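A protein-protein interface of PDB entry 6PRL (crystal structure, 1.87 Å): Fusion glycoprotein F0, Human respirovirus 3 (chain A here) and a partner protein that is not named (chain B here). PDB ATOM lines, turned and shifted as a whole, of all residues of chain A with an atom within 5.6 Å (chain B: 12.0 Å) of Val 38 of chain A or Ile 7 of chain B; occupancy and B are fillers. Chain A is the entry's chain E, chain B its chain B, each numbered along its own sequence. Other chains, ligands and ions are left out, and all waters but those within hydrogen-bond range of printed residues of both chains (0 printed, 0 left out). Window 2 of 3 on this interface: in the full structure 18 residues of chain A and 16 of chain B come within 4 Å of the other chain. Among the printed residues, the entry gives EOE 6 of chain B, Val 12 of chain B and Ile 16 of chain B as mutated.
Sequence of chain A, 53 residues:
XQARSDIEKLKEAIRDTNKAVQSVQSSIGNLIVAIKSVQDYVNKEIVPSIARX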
ATOM      1  N   VAL A  33     -13.595  -9.773 -14.438  1.00  0.00           N
ATOM      2  CA  VAL A  33     -13.615 -10.243 -15.819  1.00  0.00           C
ATOM      3  C   VAL A  33     -12.792 -11.515 -15.961  1.00  0.00           C
ATOM      4  O   VAL A  33     -13.210 -12.473 -16.630  1.00  0.00           O
ATOM      5  CB  VAL A  33     -13.100  -9.141 -16.767  1.00  0.00           C
ATOM      6  CG1 VAL A  33     -13.046  -9.664 -18.201  1.00  0.00           C
ATOM      7  CG2 VAL A  33     -13.969  -7.899 -16.671  1.00  0.00           C
ATOM      8  N   ALA A  34     -11.606 -11.543 -15.356  1.00  0.00           N
ATOM      9  CA  ALA A  34     -10.755 -12.724 -15.450  1.00  0.00           C
ATOM     10  C   ALA A  34     -11.452 -13.943 -14.860  1.00  0.00           C
ATOM     11  O   ALA A  34     -11.503 -15.007 -15.485  1.00  0.00           O
ATOM     12  CB  ALA A  34      -9.424 -12.470 -14.740  1.00  0.00           C
ATOM     13  N   ILE A  35     -11.998 -13.803 -13.649  1.00  0.00           N
ATOM     14  CA  ILE A  35     -12.650 -14.934 -12.995  1.00  0.00           C
ATOM     15  C   ILE A  35     -13.871 -15.375 -13.791  1.00  0.00           C
ATOM     16  O   ILE A  35     -14.105 -16.574 -13.982  1.00  0.00           O
ATOM     17  CB  ILE A  35     -13.019 -14.576 -11.544  1.00  0.00           C
ATOM     18  CG1 ILE A  35     -11.756 -14.276 -10.736  1.00  0.00           C
ATOM     19  CG2 ILE A  35     -13.811 -15.708 -10.904  1.00  0.00           C
ATOM     20  CD1 ILE A  35     -12.026 -13.590  -9.409  1.00  0.00           C
ATOM     21  N   LYS A  36     -14.668 -14.417 -14.271  1.00  0.00           N
ATOM     22  CA  LYS A  36     -15.854 -14.773 -15.040  1.00  0.00           C
ATOM     23  C   LYS A  36     -15.493 -15.445 -16.360  1.00  0.00           C
ATOM     24  O   LYS A  36     -16.248 -16.292 -16.847  1.00  0.00           O
ATOM     25  CB  LYS A  36     -16.716 -13.538 -15.296  1.00  0.00           C
ATOM     26  CG  LYS A  36     -17.882 -13.807 -16.232  1.00  0.00           C
ATOM     27  CD  LYS A  36     -19.012 -12.813 -16.038  1.00  0.00           C
ATOM     28  CE  LYS A  36     -20.157 -13.089 -17.005  1.00  0.00           C
ATOM     29  NZ  LYS A  36     -20.633 -14.501 -16.933  1.00  0.00           N
ATOM     30  N   SER A  37     -14.357 -15.082 -16.957  1.00  0.00           N
ATOM     31  CA  SER A  37     -13.931 -15.763 -18.178  1.00  0.00           C
ATOM     32  C   SER A  37     -13.609 -17.226 -17.904  1.00  0.00           C
ATOM     33  O   SER A  37     -13.966 -18.106 -18.698  1.00  0.00           O
ATOM     34  CB  SER A  37     -12.721 -15.050 -18.779  1.00  0.00           C
ATOM     35  OG  SER A  37     -13.053 -13.730 -19.167  1.00  0.00           O
ATOM     36  N   VAL A  38     -12.929 -17.505 -16.791  1.00  0.00           N
ATOM     37  CA  VAL A  38     -12.640 -18.888 -16.420  1.00  0.00           C
ATOM     38  C   VAL A  38     -13.938 -19.651 -16.192  1.00  0.00           C
ATOM     39  O   VAL A  38     -14.122 -20.765 -16.698  1.00  0.00           O
ATOM     40  CB  VAL A  38     -11.734 -18.929 -15.176  1.00  0.00           C
ATOM     41  CG1 VAL A  38     -11.479 -20.359 -14.747  1.00  0.00           C
ATOM     42  CG2 VAL A  38     -10.420 -18.207 -15.454  1.00  0.00           C
ATOM     43  N   GLN A  39     -14.862 -19.054 -15.433  1.00  0.00           N
ATOM     44  CA  GLN A  39     -16.162 -19.674 -15.198  1.00  0.00           C
ATOM     45  C   GLN A  39     -16.849 -20.024 -16.511  1.00  0.00           C
ATOM     46  O   GLN A  39     -17.323 -21.150 -16.699  1.00  0.00           O
ATOM     47  CB  GLN A  39     -17.041 -18.729 -14.373  1.00  0.00           C
ATOM     48  CG  GLN A  39     -18.445 -19.251 -14.084  1.00  0.00           C
ATOM     49  CD  GLN A  39     -19.445 -18.135 -13.821  1.00  0.00           C
ATOM     50  OE1 GLN A  39     -19.282 -17.014 -14.306  1.00  0.00           O
ATOM     51  NE2 GLN A  39     -20.482 -18.435 -13.054  1.00  0.00           N
ATOM     52  N   ASP A  40     -16.919 -19.060 -17.432  1.00  0.00           N
ATOM     53  CA  ASP A  40     -17.680 -19.260 -18.659  1.00  0.00           C
ATOM     54  C   ASP A  40     -17.068 -20.351 -19.525  1.00  0.00           C
ATOM     55  O   ASP A  40     -17.797 -21.156 -20.120  1.00  0.00           O
ATOM     56  CB  ASP A  40     -17.778 -17.948 -19.437  1.00  0.00           C
ATOM     57  CG  ASP A  40     -18.620 -16.905 -18.720  1.00  0.00           C
ATOM     58  OD1 ASP A  40     -19.474 -17.291 -17.892  1.00  0.00           O
ATOM     59  OD2 ASP A  40     -18.434 -15.703 -18.992  1.00  0.00           O
ATOM     60  N   TYR A  41     -15.736 -20.399 -19.618  1.00  0.00           N
ATOM     61  CA  TYR A  41     -15.105 -21.448 -20.413  1.00  0.00           C
ATOM     62  C   TYR A  41     -15.412 -22.825 -19.840  1.00  0.00           C
ATOM     63  O   TYR A  41     -15.721 -23.762 -20.587  1.00  0.00           O
ATOM     64  CB  TYR A  41     -13.596 -21.230 -20.488  1.00  0.00           C
ATOM     65  CG  TYR A  41     -12.890 -22.273 -21.320  1.00  0.00           C
ATOM     66  CD1 TYR A  41     -12.692 -22.085 -22.682  1.00  0.00           C
ATOM     67  CD2 TYR A  41     -12.431 -23.452 -20.749  1.00  0.00           C
ATOM     68  CE1 TYR A  41     -12.052 -23.044 -23.450  1.00  0.00           C
ATOM     69  CE2 TYR A  41     -11.794 -24.416 -21.509  1.00  0.00           C
ATOM     70  CZ  TYR A  41     -11.606 -24.206 -22.857  1.00  0.00           C
ATOM     71  OH  TYR A  41     -10.970 -25.163 -23.615  1.00  0.00           O
ATOM     72  N   VAL A  42     -15.329 -22.970 -18.517  1.00  0.00           N
ATOM     73  CA  VAL A  42     -15.618 -24.260 -17.891  1.00  0.00           C
ATOM     74  C   VAL A  42     -17.048 -24.685 -18.194  1.00  0.00           C
ATOM     75  O   VAL A  42     -17.311 -25.839 -18.555  1.00  0.00           O
ATOM     76  CB  VAL A  42     -15.362 -24.183 -16.374  1.00  0.00           C
ATOM     77  CG1 VAL A  42     -15.850 -25.443 -15.681  1.00  0.00           C
ATOM     78  CG2 VAL A  42     -13.883 -23.955 -16.099  1.00  0.00           C
ATOM     79  N   ASN A  43     -17.995 -23.754 -18.062  1.00  0.00           N
ATOM     80  CA  ASN A  43     -19.401 -24.090 -18.233  1.00  0.00           C
ATOM     81  C   ASN A  43     -19.745 -24.380 -19.688  1.00  0.00           C
ATOM     82  O   ASN A  43     -20.601 -25.229 -19.961  1.00  0.00           O
ATOM     83  CB  ASN A  43     -20.276 -22.952 -17.704  1.00  0.00           C
ATOM     84  CG  ASN A  43     -20.222 -22.829 -16.193  1.00  0.00           C
ATOM     85  OD1 ASN A  43     -20.024 -23.814 -15.485  1.00  0.00           O
ATOM     86  ND2 ASN A  43     -20.402 -21.615 -15.693  1.00  0.00           N
ATOM     87  N   ASP B   5      -3.991 -19.513 -25.652  1.00  0.00           N
ATOM     88  CA  ASP B   5      -4.261 -20.611 -24.723  1.00  0.00           C
ATOM     89  C   ASP B   5      -5.662 -21.176 -24.953  1.00  0.00           C
ATOM     90  O   ASP B   5      -6.601 -20.417 -25.191  1.00  0.00           O
ATOM     91  CB  ASP B   5      -4.119 -20.137 -23.272  1.00  0.00           C
ATOM     92  CG  ASP B   5      -2.687 -19.829 -22.894  1.00  0.00           C
ATOM     93  OD1 ASP B   5      -2.415 -18.686 -22.472  1.00  0.00           O
ATOM     94  OD2 ASP B   5      -1.831 -20.729 -23.029  1.00  0.00           O
ATOM     95  C   EOE B   6      -8.429 -21.917 -23.219  1.00  0.00           C
ATOM     96  CA  EOE B   6      -8.029 -23.319 -23.768  1.00  0.00           C
ATOM     97  CB  EOE B   6      -7.250 -23.218 -25.109  1.00  0.00           C
ATOM     98  C05 EOE B   6      -6.988 -24.406 -25.568  1.00  0.00           C
ATOM     99  C06 EOE B   6      -5.593 -24.770 -25.008  1.00  0.00           C
ATOM    100  C07 EOE B   6      -4.926 -23.427 -24.642  1.00  0.00           C
ATOM    101  N   EOE B   6      -5.814 -22.499 -24.885  1.00  0.00           N
ATOM    102  O   EOE B   6      -9.002 -21.083 -23.965  1.00  0.00           O
ATOM    103  N   ILE B   7      -8.133 -21.670 -21.949  1.00  0.00           N
ATOM    104  CA  ILE B   7      -8.455 -20.395 -21.323  1.00  0.00           C
ATOM    105  C   ILE B   7      -7.296 -19.437 -21.573  1.00  0.00           C
ATOM    106  O   ILE B   7      -6.148 -19.763 -21.276  1.00  0.00           O
ATOM    107  CB  ILE B   7      -8.720 -20.545 -19.822  1.00  0.00           C
ATOM    108  CG1 ILE B   7      -9.739 -21.653 -19.565  1.00  0.00           C
ATOM    109  CG2 ILE B   7      -9.226 -19.230 -19.239  1.00  0.00           C
ATOM    110  CD1 ILE B   7      -9.980 -21.926 -18.096  1.00  0.00           C
ATOM    111  N   ASP B   8      -7.602 -18.259 -22.112  1.00  0.00           N
ATOM    112  CA  ASP B   8      -6.606 -17.217 -22.344  1.00  0.00           C
ATOM    113  C   ASP B   8      -7.114 -15.932 -21.705  1.00  0.00           C
ATOM    114  O   ASP B   8      -8.050 -15.307 -22.217  1.00  0.00           O
ATOM    115  CB  ASP B   8      -6.343 -17.015 -23.838  1.00  0.00           C
ATOM    116  CG  ASP B   8      -5.226 -16.017 -24.107  1.00  0.00           C
ATOM    117  OD1 ASP B   8      -5.256 -14.906 -23.534  1.00  0.00           O
ATOM    118  OD2 ASP B   8      -4.311 -16.347 -24.892  1.00  0.00           O
ATOM    119  N   ILE B   9      -6.503 -15.546 -20.588  1.00  0.00           N
ATOM    120  CA  ILE B   9      -6.851 -14.306 -19.904  1.00  0.00           C
ATOM    121  C   ILE B   9      -5.612 -13.423 -19.826  1.00  0.00           C
ATOM    122  O   ILE B   9      -5.440 -12.660 -18.869  1.00  0.00           O
ATOM    123  CB  ILE B   9      -7.427 -14.579 -18.502  1.00  0.00           C
ATOM    124  CG1 ILE B   9      -6.523 -15.541 -17.729  1.00  0.00           C
ATOM    125  CG2 ILE B   9      -8.843 -15.131 -18.611  1.00  0.00           C
ATOM    126  CD1 ILE B   9      -6.968 -15.786 -16.302  1.00  0.00           C
ATOM    127  N   SER B  10      -4.749 -13.513 -20.842  1.00  0.00           N
ATOM    128  CA  SER B  10      -3.504 -12.752 -20.836  1.00  0.00           C
ATOM    129  C   SER B  10      -3.762 -11.253 -20.925  1.00  0.00           C
ATOM    130  O   SER B  10      -3.101 -10.462 -20.241  1.00  0.00           O
ATOM    131  CB  SER B  10      -2.615 -13.203 -21.994  1.00  0.00           C
ATOM    132  OG  SER B  10      -3.210 -12.879 -23.241  1.00  0.00           O
ATOM    133  N   ILE B  11      -4.706 -10.840 -21.772  1.00  0.00           N
ATOM    134  CA  ILE B  11      -4.995  -9.417 -21.928  1.00  0.00           C
ATOM    135  C   ILE B  11      -5.417  -8.813 -20.595  1.00  0.00           C
ATOM    136  O   ILE B  11      -4.900  -7.771 -20.172  1.00  0.00           O
ATOM    137  CB  ILE B  11      -6.074  -9.205 -23.007  1.00  0.00           C
ATOM    138  CG1 ILE B  11      -5.522  -9.534 -24.398  1.00  0.00           C
ATOM    139  CG2 ILE B  11      -6.611  -7.776 -22.953  1.00  0.00           C
ATOM    140  CD1 ILE B  11      -4.382  -8.635 -24.848  1.00  0.00           C
ATOM    141  N   VAL B  12      -6.362  -9.458 -19.909  1.00  0.00           N
ATOM    142  CA  VAL B  12      -6.920  -8.872 -18.696  1.00  0.00           C
ATOM    143  C   VAL B  12      -5.907  -8.919 -17.558  1.00  0.00           C
ATOM    144  O   VAL B  12      -5.778  -7.960 -16.787  1.00  0.00           O
ATOM    145  CB  VAL B  12      -8.240  -9.579 -18.325  1.00  0.00           C
ATOM    146  CG1 VAL B  12      -8.013 -11.056 -18.043  1.00  0.00           C
ATOM    147  CG2 VAL B  12      -8.885  -8.894 -17.127  1.00  0.00           C
ATOM    148  N   LEU B  13      -5.171 -10.026 -17.427  1.00  0.00           N
ATOM    149  CA  LEU B  13      -4.183 -10.110 -16.355  1.00  0.00           C
ATOM    150  C   LEU B  13      -3.068  -9.088 -16.555  1.00  0.00           C
ATOM    151  O   LEU B  13      -2.578  -8.498 -15.583  1.00  0.00           O
ATOM    152  CB  LEU B  13      -3.611 -11.524 -16.263  1.00  0.00           C
ATOM    153  CG  LEU B  13      -4.564 -12.620 -15.785  1.00  0.00           C
ATOM    154  CD1 LEU B  13      -3.819 -13.940 -15.623  1.00  0.00           C
ATOM    155  CD2 LEU B  13      -5.251 -12.238 -14.485  1.00  0.00           C
ATOM    156  N   ASN B  14      -2.661  -8.853 -17.806  1.00  0.00           N
ATOM    157  CA  ASN B  14      -1.652  -7.833 -18.074  1.00  0.00           C
ATOM    158  C   ASN B  14      -2.165  -6.445 -17.712  1.00  0.00           C
ATOM    159  O   ASN B  14      -1.407  -5.600 -17.222  1.00  0.00           O
ATOM    160  CB  ASN B  14      -1.235  -7.873 -19.544  1.00  0.00           C
ATOM    161  CG  ASN B  14      -0.442  -9.115 -19.891  1.00  0.00           C
ATOM    162  OD1 ASN B  14       0.153  -9.751 -19.020  1.00  0.00           O
ATOM    163  ND2 ASN B  14      -0.422  -9.465 -21.173  1.00  0.00           N
ATOM    164  N   ILE B  16      -4.305  -5.820 -15.338  1.00  0.00           N
ATOM    165  CA  ILE B  16      -4.327  -5.745 -13.879  1.00  0.00           C
ATOM    166  C   ILE B  16      -2.943  -5.404 -13.344  1.00  0.00           C
ATOM    167  O   ILE B  16      -2.787  -4.528 -12.483  1.00  0.00           O
ATOM    168  CB  ILE B  16      -4.847  -7.065 -13.279  1.00  0.00           C
ATOM    169  CG1 ILE B  16      -6.302  -7.301 -13.679  1.00  0.00           C
ATOM    170  CG2 ILE B  16      -4.703  -7.035 -11.763  1.00  0.00           C
ATOM    171  CD1 ILE B  16      -6.775  -8.720 -13.445  1.00  0.00           C
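The backbone carbonyl oxygen (O) of Val 33 of chain A lies within hydrogen-bond range of the side-chain hydroxyl (OG) of Ser 37 of chain A, at 2.8 Å.
Among the printed residues, pairs that only touch across the chains: Tyr 41 of chain A with Ile 7 of chain B (3.4 Å), Tyr 41 of chain A with EOE 6 of chain B (3.5 Å), Ala 34 of chain A with Val 12 of chain B (3.9 Å), Ser 37 of chain A with Ile 9 of chain B (3.9 Å) and Val 38 of chain A with Ile 7 of chain B (3.99 Å).
Printed residues of chain B within 4 Å of Val 38 of chain A: Ile 7 (3.99 Å).
Printed residues of chain A within 4 Å of Ile 7 of chain B: Val 38 and Tyr 41.
Ala 34 of chain A touches just one residue of chain B: Val 12 (3.9 Å).
No residue of chain B comes within 4 Å of Ile 35 of chain A.
Of chain B, only Ile 9 (3.9 Å) comes within 4 Å of Ser 37 of chain A.
No residue of chain B comes within 4 Å of Asp 40 of chain A.
No residue of chain B comes within 4 Å of Val 42 of chain A.
Of the printed residues of chain A, Ile 9 of chain B touches Ser 37 (3.9 Å).
Of the printed residues of chain A, EOE 6 of chain B touches Tyr 41 (3.5 Å).
Printed residues of chain A within 4 Å of Val 12 of chain B: Ala 34.
Asp 5 of chain B touches none of the printed residues of chain A.
Of the 11 printed residues of chain A, 4 touch a printed residue of chain B.
Printed residues of chain A that touch a printed residue of chain B: Ala 34, Ser 37, Val 38 and Tyr 41.
Hydrophobic or aromatic side chains of chain A within 4 Å of the printed part of chain B: Ala 34, Val 38 and Tyr 41.
Along chain A the printed residues that touch a printed residue of chain B span positions 34 to 41.
Printed residues of chain B that touch a printed residue of chain A: EOE 6, Ile 7, Ile 9 and Val 12.
Hydrophobic or aromatic side chains of chain B within 4 Å of the printed part of chain A: Ile 7, Ile 9 and Val 12.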
